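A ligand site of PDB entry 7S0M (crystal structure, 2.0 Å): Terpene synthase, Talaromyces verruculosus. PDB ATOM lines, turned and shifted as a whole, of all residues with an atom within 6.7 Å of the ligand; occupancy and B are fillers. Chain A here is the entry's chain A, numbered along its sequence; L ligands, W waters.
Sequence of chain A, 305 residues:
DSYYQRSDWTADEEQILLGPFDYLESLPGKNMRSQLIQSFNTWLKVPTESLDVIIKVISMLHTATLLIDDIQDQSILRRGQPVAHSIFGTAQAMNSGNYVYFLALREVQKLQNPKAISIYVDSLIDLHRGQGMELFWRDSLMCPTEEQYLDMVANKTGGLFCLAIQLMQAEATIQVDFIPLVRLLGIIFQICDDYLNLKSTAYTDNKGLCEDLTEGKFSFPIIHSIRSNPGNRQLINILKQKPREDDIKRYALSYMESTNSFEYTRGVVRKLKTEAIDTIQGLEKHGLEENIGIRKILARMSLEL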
ATOM      1  N   LEU A  27     -27.786  15.017  11.116  1.00  0.00           N
ATOM      2  CA  LEU A  27     -26.979  14.053  10.378  1.00  0.00           C
ATOM      3  C   LEU A  27     -27.245  12.645  10.881  1.00  0.00           C
ATOM      4  O   LEU A  27     -27.109  12.392  12.091  1.00  0.00           O
ATOM      5  CB  LEU A  27     -25.506  14.363  10.507  1.00  0.00           C
ATOM      6  CG  LEU A  27     -25.021  15.781  10.169  1.00  0.00           C
ATOM      7  CD1 LEU A  27     -23.523  15.859  10.353  1.00  0.00           C
ATOM      8  CD2 LEU A  27     -25.426  16.174   8.751  1.00  0.00           C
ATOM      9  N   PRO A  28     -27.586  11.693   9.995  1.00  0.00           N
ATOM     10  CA  PRO A  28     -28.004  10.360  10.458  1.00  0.00           C
ATOM     11  C   PRO A  28     -26.843   9.576  11.051  1.00  0.00           C
ATOM     12  O   PRO A  28     -25.799   9.422  10.413  1.00  0.00           O
ATOM     13  CB  PRO A  28     -28.541   9.685   9.189  1.00  0.00           C
ATOM     14  CG  PRO A  28     -28.568  10.739   8.123  1.00  0.00           C
ATOM     15  CD  PRO A  28     -27.578  11.797   8.535  1.00  0.00           C
ATOM     16  N   GLY A  29     -27.028   9.111  12.282  1.00  0.00           N
ATOM     17  CA  GLY A  29     -26.111   8.211  12.933  1.00  0.00           C
ATOM     18  C   GLY A  29     -26.635   6.781  12.976  1.00  0.00           C
ATOM     19  O   GLY A  29     -27.666   6.452  12.387  1.00  0.00           O
ATOM     20  N   LYS A  30     -25.901   5.928  13.690  1.00  0.00           N
ATOM     21  CA  LYS A  30     -26.241   4.510  13.752  1.00  0.00           C
ATOM     22  C   LYS A  30     -27.142   4.128  14.926  1.00  0.00           C
ATOM     23  O   LYS A  30     -27.750   3.054  14.889  1.00  0.00           O
ATOM     24  CB  LYS A  30     -24.979   3.632  13.807  1.00  0.00           C
ATOM     25  CG  LYS A  30     -23.939   3.918  12.739  1.00  0.00           C
ATOM     26  CD  LYS A  30     -22.627   3.228  13.075  1.00  0.00           C
ATOM     27  CE  LYS A  30     -21.570   4.212  13.530  1.00  0.00           C
ATOM     28  NZ  LYS A  30     -20.879   3.751  14.764  1.00  0.00           N
ATOM     29  N   ASN A  31     -27.221   4.960  15.953  1.00  0.00           N
ATOM     30  CA  ASN A  31     -28.148   4.752  17.074  1.00  0.00           C
ATOM     31  C   ASN A  31     -27.828   3.483  17.856  1.00  0.00           C
ATOM     32  O   ASN A  31     -28.715   2.763  18.317  1.00  0.00           O
ATOM     33  CB  ASN A  31     -29.596   4.732  16.589  1.00  0.00           C
ATOM     34  CG  ASN A  31     -30.264   6.068  16.767  1.00  0.00           C
ATOM     35  OD1 ASN A  31     -30.670   6.412  17.875  1.00  0.00           O
ATOM     36  ND2 ASN A  31     -30.347   6.835  15.688  1.00  0.00           N
ATOM     37  N   MET A  32     -26.538   3.231  18.027  1.00  0.00           N
ATOM     38  CA  MET A  32     -26.101   2.101  18.837  1.00  0.00           C
ATOM     39  C   MET A  32     -26.590   2.236  20.276  1.00  0.00           C
ATOM     40  O   MET A  32     -27.071   1.273  20.879  1.00  0.00           O
ATOM     41  CB  MET A  32     -24.583   1.989  18.782  1.00  0.00           C
ATOM     42  CG  MET A  32     -23.969   1.110  19.854  1.00  0.00           C
ATOM     43  SD  MET A  32     -24.032  -0.638  19.373  1.00  0.00           S
ATOM     44  CE  MET A  32     -23.926  -0.509  17.585  1.00  0.00           C
ATOM     45  N   ARG A  33     -26.443   3.436  20.861  1.00  0.00           N
ATOM     46  CA  ARG A  33     -26.772   3.590  22.276  1.00  0.00           C
ATOM     47  C   ARG A  33     -28.258   3.403  22.529  1.00  0.00           C
ATOM     48  O   ARG A  33     -28.651   2.873  23.569  1.00  0.00           O
ATOM     49  CB  ARG A  33     -26.266   4.949  22.796  1.00  0.00           C
ATOM     50  CG  ARG A  33     -24.737   4.982  23.029  1.00  0.00           C
ATOM     51  CD  ARG A  33     -24.150   6.405  23.038  1.00  0.00           C
ATOM     52  NE  ARG A  33     -22.689   6.394  23.033  1.00  0.00           N
ATOM     53  CZ  ARG A  33     -21.934   6.191  21.955  1.00  0.00           C
ATOM     54  NH1 ARG A  33     -22.478   5.994  20.766  1.00  0.00           N
ATOM     55  NH2 ARG A  33     -20.612   6.181  22.072  1.00  0.00           N
ATOM     56  N   SER A  34     -29.101   3.786  21.568  1.00  0.00           N
ATOM     57  CA  SER A  34     -30.531   3.522  21.724  1.00  0.00           C
ATOM     58  C   SER A  34     -30.828   2.032  21.710  1.00  0.00           C
ATOM     59  O   SER A  34     -31.613   1.547  22.530  1.00  0.00           O
ATOM     60  CB  SER A  34     -31.305   4.249  20.634  1.00  0.00           C
ATOM     61  OG  SER A  34     -31.463   5.615  20.986  1.00  0.00           O
ATOM     62  N   ILE A  58     -29.139  10.685  27.002  1.00  0.00           N
ATOM     63  CA  ILE A  58     -27.982  10.023  26.405  1.00  0.00           C
ATOM     64  C   ILE A  58     -27.716  10.530  24.989  1.00  0.00           C
ATOM     65  O   ILE A  58     -26.568  10.724  24.595  1.00  0.00           O
ATOM     66  CB  ILE A  58     -28.177   8.488  26.427  1.00  0.00           C
ATOM     67  CG1 ILE A  58     -28.183   7.971  27.870  1.00  0.00           C
ATOM     68  CG2 ILE A  58     -27.072   7.794  25.683  1.00  0.00           C
ATOM     69  CD1 ILE A  58     -26.920   8.279  28.620  1.00  0.00           C
ATOM     70  N   HIS A  62     -24.353  12.439  23.953  1.00  0.00           N
ATOM     71  CA  HIS A  62     -23.554  11.844  22.871  1.00  0.00           C
ATOM     72  C   HIS A  62     -23.245  12.886  21.803  1.00  0.00           C
ATOM     73  O   HIS A  62     -22.086  13.064  21.419  1.00  0.00           O
ATOM     74  CB  HIS A  62     -24.291  10.650  22.257  1.00  0.00           C
ATOM     75  CG  HIS A  62     -23.556  10.039  21.101  1.00  0.00           C
ATOM     76  ND1 HIS A  62     -22.249   9.604  21.192  1.00  0.00           N
ATOM     77  CD2 HIS A  62     -23.946   9.806  19.822  1.00  0.00           C
ATOM     78  CE1 HIS A  62     -21.874   9.109  20.031  1.00  0.00           C
ATOM     79  NE2 HIS A  62     -22.879   9.221  19.174  1.00  0.00           N
ATOM     80  N   LEU A  66     -19.584  14.585  20.723  1.00  0.00           N
ATOM     81  CA  LEU A  66     -19.025  14.560  19.376  1.00  0.00           C
ATOM     82  C   LEU A  66     -18.591  15.958  18.945  1.00  0.00           C
ATOM     83  O   LEU A  66     -17.526  16.119  18.325  1.00  0.00           O
ATOM     84  CB  LEU A  66     -20.050  14.014  18.386  1.00  0.00           C
ATOM     85  CG  LEU A  66     -20.557  12.590  18.611  1.00  0.00           C
ATOM     86  CD1 LEU A  66     -21.507  12.187  17.507  1.00  0.00           C
ATOM     87  CD2 LEU A  66     -19.397  11.640  18.699  1.00  0.00           C
ATOM     88  N   ARG A  78     -17.508  14.244   9.851  1.00  0.00           N
ATOM     89  CA  ARG A  78     -18.263  13.540  10.874  1.00  0.00           C
ATOM     90  C   ARG A  78     -19.548  13.064  10.219  1.00  0.00           C
ATOM     91  O   ARG A  78     -20.269  13.868   9.622  1.00  0.00           O
ATOM     92  CB  ARG A  78     -18.566  14.443  12.078  1.00  0.00           C
ATOM     93  CG  ARG A  78     -19.799  14.027  12.888  1.00  0.00           C
ATOM     94  CD  ARG A  78     -19.518  12.791  13.723  1.00  0.00           C
ATOM     95  NE  ARG A  78     -18.349  12.995  14.571  1.00  0.00           N
ATOM     96  CZ  ARG A  78     -17.757  12.052  15.281  1.00  0.00           C
ATOM     97  NH1 ARG A  78     -18.201  10.805  15.259  1.00  0.00           N
ATOM     98  NH2 ARG A  78     -16.689  12.358  16.008  1.00  0.00           N
ATOM     99  N   ARG A  79     -19.812  11.756  10.303  1.00  0.00           N
ATOM    100  CA  ARG A  79     -20.926  11.134   9.576  1.00  0.00           C
ATOM    101  C   ARG A  79     -20.903  11.507   8.090  1.00  0.00           C
ATOM    102  O   ARG A  79     -21.934  11.730   7.470  1.00  0.00           O
ATOM    103  CB  ARG A  79     -22.276  11.503  10.207  1.00  0.00           C
ATOM    104  CG  ARG A  79     -22.446  10.958  11.639  1.00  0.00           C
ATOM    105  CD  ARG A  79     -23.584  11.646  12.411  1.00  0.00           C
ATOM    106  NE  ARG A  79     -23.656  11.121  13.774  1.00  0.00           N
ATOM    107  CZ  ARG A  79     -24.439  11.594  14.738  1.00  0.00           C
ATOM    108  NH1 ARG A  79     -25.212  12.651  14.545  1.00  0.00           N
ATOM    109  NH2 ARG A  79     -24.457  10.978  15.922  1.00  0.00           N
ATOM    110  N   PHE A 161     -21.952   4.713  28.120  1.00  0.00           N
ATOM    111  CA  PHE A 161     -22.630   3.423  28.197  1.00  0.00           C
ATOM    112  C   PHE A 161     -23.098   3.171  29.626  1.00  0.00           C
ATOM    113  O   PHE A 161     -24.258   2.823  29.876  1.00  0.00           O
ATOM    114  CB  PHE A 161     -21.689   2.291  27.788  1.00  0.00           C
ATOM    115  CG  PHE A 161     -21.553   2.100  26.290  1.00  0.00           C
ATOM    116  CD1 PHE A 161     -21.193   3.146  25.467  1.00  0.00           C
ATOM    117  CD2 PHE A 161     -21.713   0.840  25.733  1.00  0.00           C
ATOM    118  CE1 PHE A 161     -21.027   2.954  24.101  1.00  0.00           C
ATOM    119  CE2 PHE A 161     -21.564   0.636  24.359  1.00  0.00           C
ATOM    120  CZ  PHE A 161     -21.220   1.700  23.542  1.00  0.00           C
ATOM    121  N   PHE A 189     -16.764  -1.815  22.110  1.00  0.00           N
ATOM    122  CA  PHE A 189     -17.195  -0.872  21.079  1.00  0.00           C
ATOM    123  C   PHE A 189     -16.070   0.076  20.682  1.00  0.00           C
ATOM    124  O   PHE A 189     -15.897   0.390  19.503  1.00  0.00           O
ATOM    125  CB  PHE A 189     -18.409  -0.084  21.599  1.00  0.00           C
ATOM    126  CG  PHE A 189     -18.964   0.885  20.602  1.00  0.00           C
ATOM    127  CD1 PHE A 189     -19.864   0.463  19.637  1.00  0.00           C
ATOM    128  CD2 PHE A 189     -18.614   2.231  20.636  1.00  0.00           C
ATOM    129  CE1 PHE A 189     -20.388   1.360  18.704  1.00  0.00           C
ATOM    130  CE2 PHE A 189     -19.137   3.121  19.710  1.00  0.00           C
ATOM    131  CZ  PHE A 189     -20.030   2.682  18.743  1.00  0.00           C
ATOM    132  N   ASP A 193     -14.115   0.446  17.196  1.00  0.00           N
ATOM    133  CA  ASP A 193     -14.031   1.754  16.560  1.00  0.00           C
ATOM    134  C   ASP A 193     -12.595   2.082  16.158  1.00  0.00           C
ATOM    135  O   ASP A 193     -12.348   2.568  15.046  1.00  0.00           O
ATOM    136  CB  ASP A 193     -14.597   2.806  17.507  1.00  0.00           C
ATOM    137  CG  ASP A 193     -14.759   4.149  16.837  1.00  0.00           C
ATOM    138  OD1 ASP A 193     -15.704   4.304  16.026  1.00  0.00           O
ATOM    139  OD2 ASP A 193     -13.937   5.048  17.127  1.00  0.00           O
ATOM    140  N   TYR A 203     -15.938   3.788   7.205  1.00  0.00           N
ATOM    141  CA  TYR A 203     -15.315   4.754   8.109  1.00  0.00           C
ATOM    142  C   TYR A 203     -14.433   5.737   7.343  1.00  0.00           C
ATOM    143  O   TYR A 203     -14.322   6.906   7.738  1.00  0.00           O
ATOM    144  CB  TYR A 203     -14.527   4.032   9.202  1.00  0.00           C
ATOM    145  CG  TYR A 203     -15.391   3.614  10.378  1.00  0.00           C
ATOM    146  CD1 TYR A 203     -16.472   2.737  10.195  1.00  0.00           C
ATOM    147  CD2 TYR A 203     -15.152   4.093  11.666  1.00  0.00           C
ATOM    148  CE1 TYR A 203     -17.278   2.356  11.242  1.00  0.00           C
ATOM    149  CE2 TYR A 203     -15.956   3.707  12.750  1.00  0.00           C
ATOM    150  CZ  TYR A 203     -17.030   2.833  12.527  1.00  0.00           C
ATOM    151  OH  TYR A 203     -17.858   2.432  13.559  1.00  0.00           O
ATOM    152  N   ASN A 206     -16.802   8.201   6.155  1.00  0.00           N
ATOM    153  CA  ASN A 206     -17.451   8.948   7.229  1.00  0.00           C
ATOM    154  C   ASN A 206     -16.518   9.979   7.876  1.00  0.00           C
ATOM    155  O   ASN A 206     -17.000  11.035   8.298  1.00  0.00           O
ATOM    156  CB  ASN A 206     -17.952   8.001   8.310  1.00  0.00           C
ATOM    157  CG  ASN A 206     -19.346   7.499   8.039  1.00  0.00           C
ATOM    158  OD1 ASN A 206     -20.017   7.945   7.094  1.00  0.00           O
ATOM    159  ND2 ASN A 206     -19.793   6.546   8.840  1.00  0.00           N
ATOM    160  N   ARG A 300     -23.361  -7.066  16.485  1.00  0.00           N
ATOM    161  CA  ARG A 300     -23.362  -5.972  15.521  1.00  0.00           C
ATOM    162  C   ARG A 300     -22.164  -5.059  15.703  1.00  0.00           C
ATOM    163  O   ARG A 300     -21.580  -4.589  14.711  1.00  0.00           O
ATOM    164  CB  ARG A 300     -24.671  -5.185  15.653  1.00  0.00           C
ATOM    165  CG  ARG A 300     -24.811  -3.982  14.749  1.00  0.00           C
ATOM    166  CD  ARG A 300     -26.140  -3.294  15.026  1.00  0.00           C
ATOM    167  NE  ARG A 300     -26.565  -2.406  13.957  1.00  0.00           N
ATOM    168  CZ  ARG A 300     -26.611  -1.083  14.054  1.00  0.00           C
ATOM    169  NH1 ARG A 300     -27.030  -0.320  13.044  1.00  0.00           N
ATOM    170  NH2 ARG A 300     -26.242  -0.490  15.191  1.00  0.00           N
HETATM  171  C1  LIG L   1     -25.044   7.784  16.205  1.00  0.00           C
HETATM  172  O1  LIG L   1     -23.772   8.225  16.592  1.00  0.00           O
HETATM  173  C2  LIG L   1     -25.857   7.375  17.421  1.00  0.00           C
HETATM  174  C3  LIG L   1     -25.158   6.220  18.161  1.00  0.00           C
HETATM  175  C4  LIG L   1     -24.365   5.335  17.540  1.00  0.00           C
HETATM  176  C5  LIG L   1     -25.416   6.108  19.658  1.00  0.00           C
HETATM  177  P1  LIG L   1     -22.548   7.651  15.664  1.00  0.00           P
HETATM  178  O2  LIG L   1     -22.951   6.260  15.234  1.00  0.00           O
HETATM  179  O3  LIG L   1     -22.378   8.532  14.440  1.00  0.00           O
HETATM  180  O4  LIG L   1     -21.140   7.632  16.522  1.00  0.00           O
HETATM  181  P2  LIG L   1     -20.538   6.329  17.347  1.00  0.00           P
HETATM  182  O5  LIG L   1     -21.624   5.559  18.059  1.00  0.00           O
HETATM  183  O6  LIG L   1     -19.836   5.421  16.360  1.00  0.00           O
HETATM  184  O7  LIG L   1     -19.564   6.859  18.387  1.00  0.00           O
HETATM  185  O   HOH W   1     -22.244   7.270  12.063  1.00  0.00           O
HETATM  186  O   HOH W   2     -20.064   9.202  14.109  1.00  0.00           O
HETATM  187  O   HOH W   3     -16.627   5.602  19.800  1.00  0.00           O
HETATM  188  O   HOH W   4     -27.374   8.091  21.374  1.00  0.00           O
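Gly 29 touches the ligand.
Asn 31 touches the ligand (N to C2, 3.1 Å).
Met 32 touches the ligand.
Phe 189 touches the ligand.
The guanidinium group (NH1) of Arg 33 is in salt-bridge range of an oxygen (O5) of the ligand.
O2 of the ligand lies close to N of Lys 30 (3.3 Å).
The guanidinium group (NE) of Arg 79 lies within salt-bridge range of an oxygen (O3) of the ligand (3.0 Å).
NZ of Lys 30 is in salt-bridge range of O6 of the ligand (2.5 Å).
NE2 of His 62 lies within hydrogen-bond range of O1 of the ligand, 2.9 Å away.
The side-chain hydroxyl (OG) of Ser 34 is in hydrogen-bond range of the side-chain amide oxygen (OD1) of Asn 31, 3.3 Å away.
The backbone carbonyl oxygen (O) of Leu 27 lies within hydrogen-bond range of the guanidinium group (NH1) of Arg 79, at 3.1 Å.
Water W2 lies within hydrogen-bond range of O3 of the ligand and NH1 of Arg 78.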
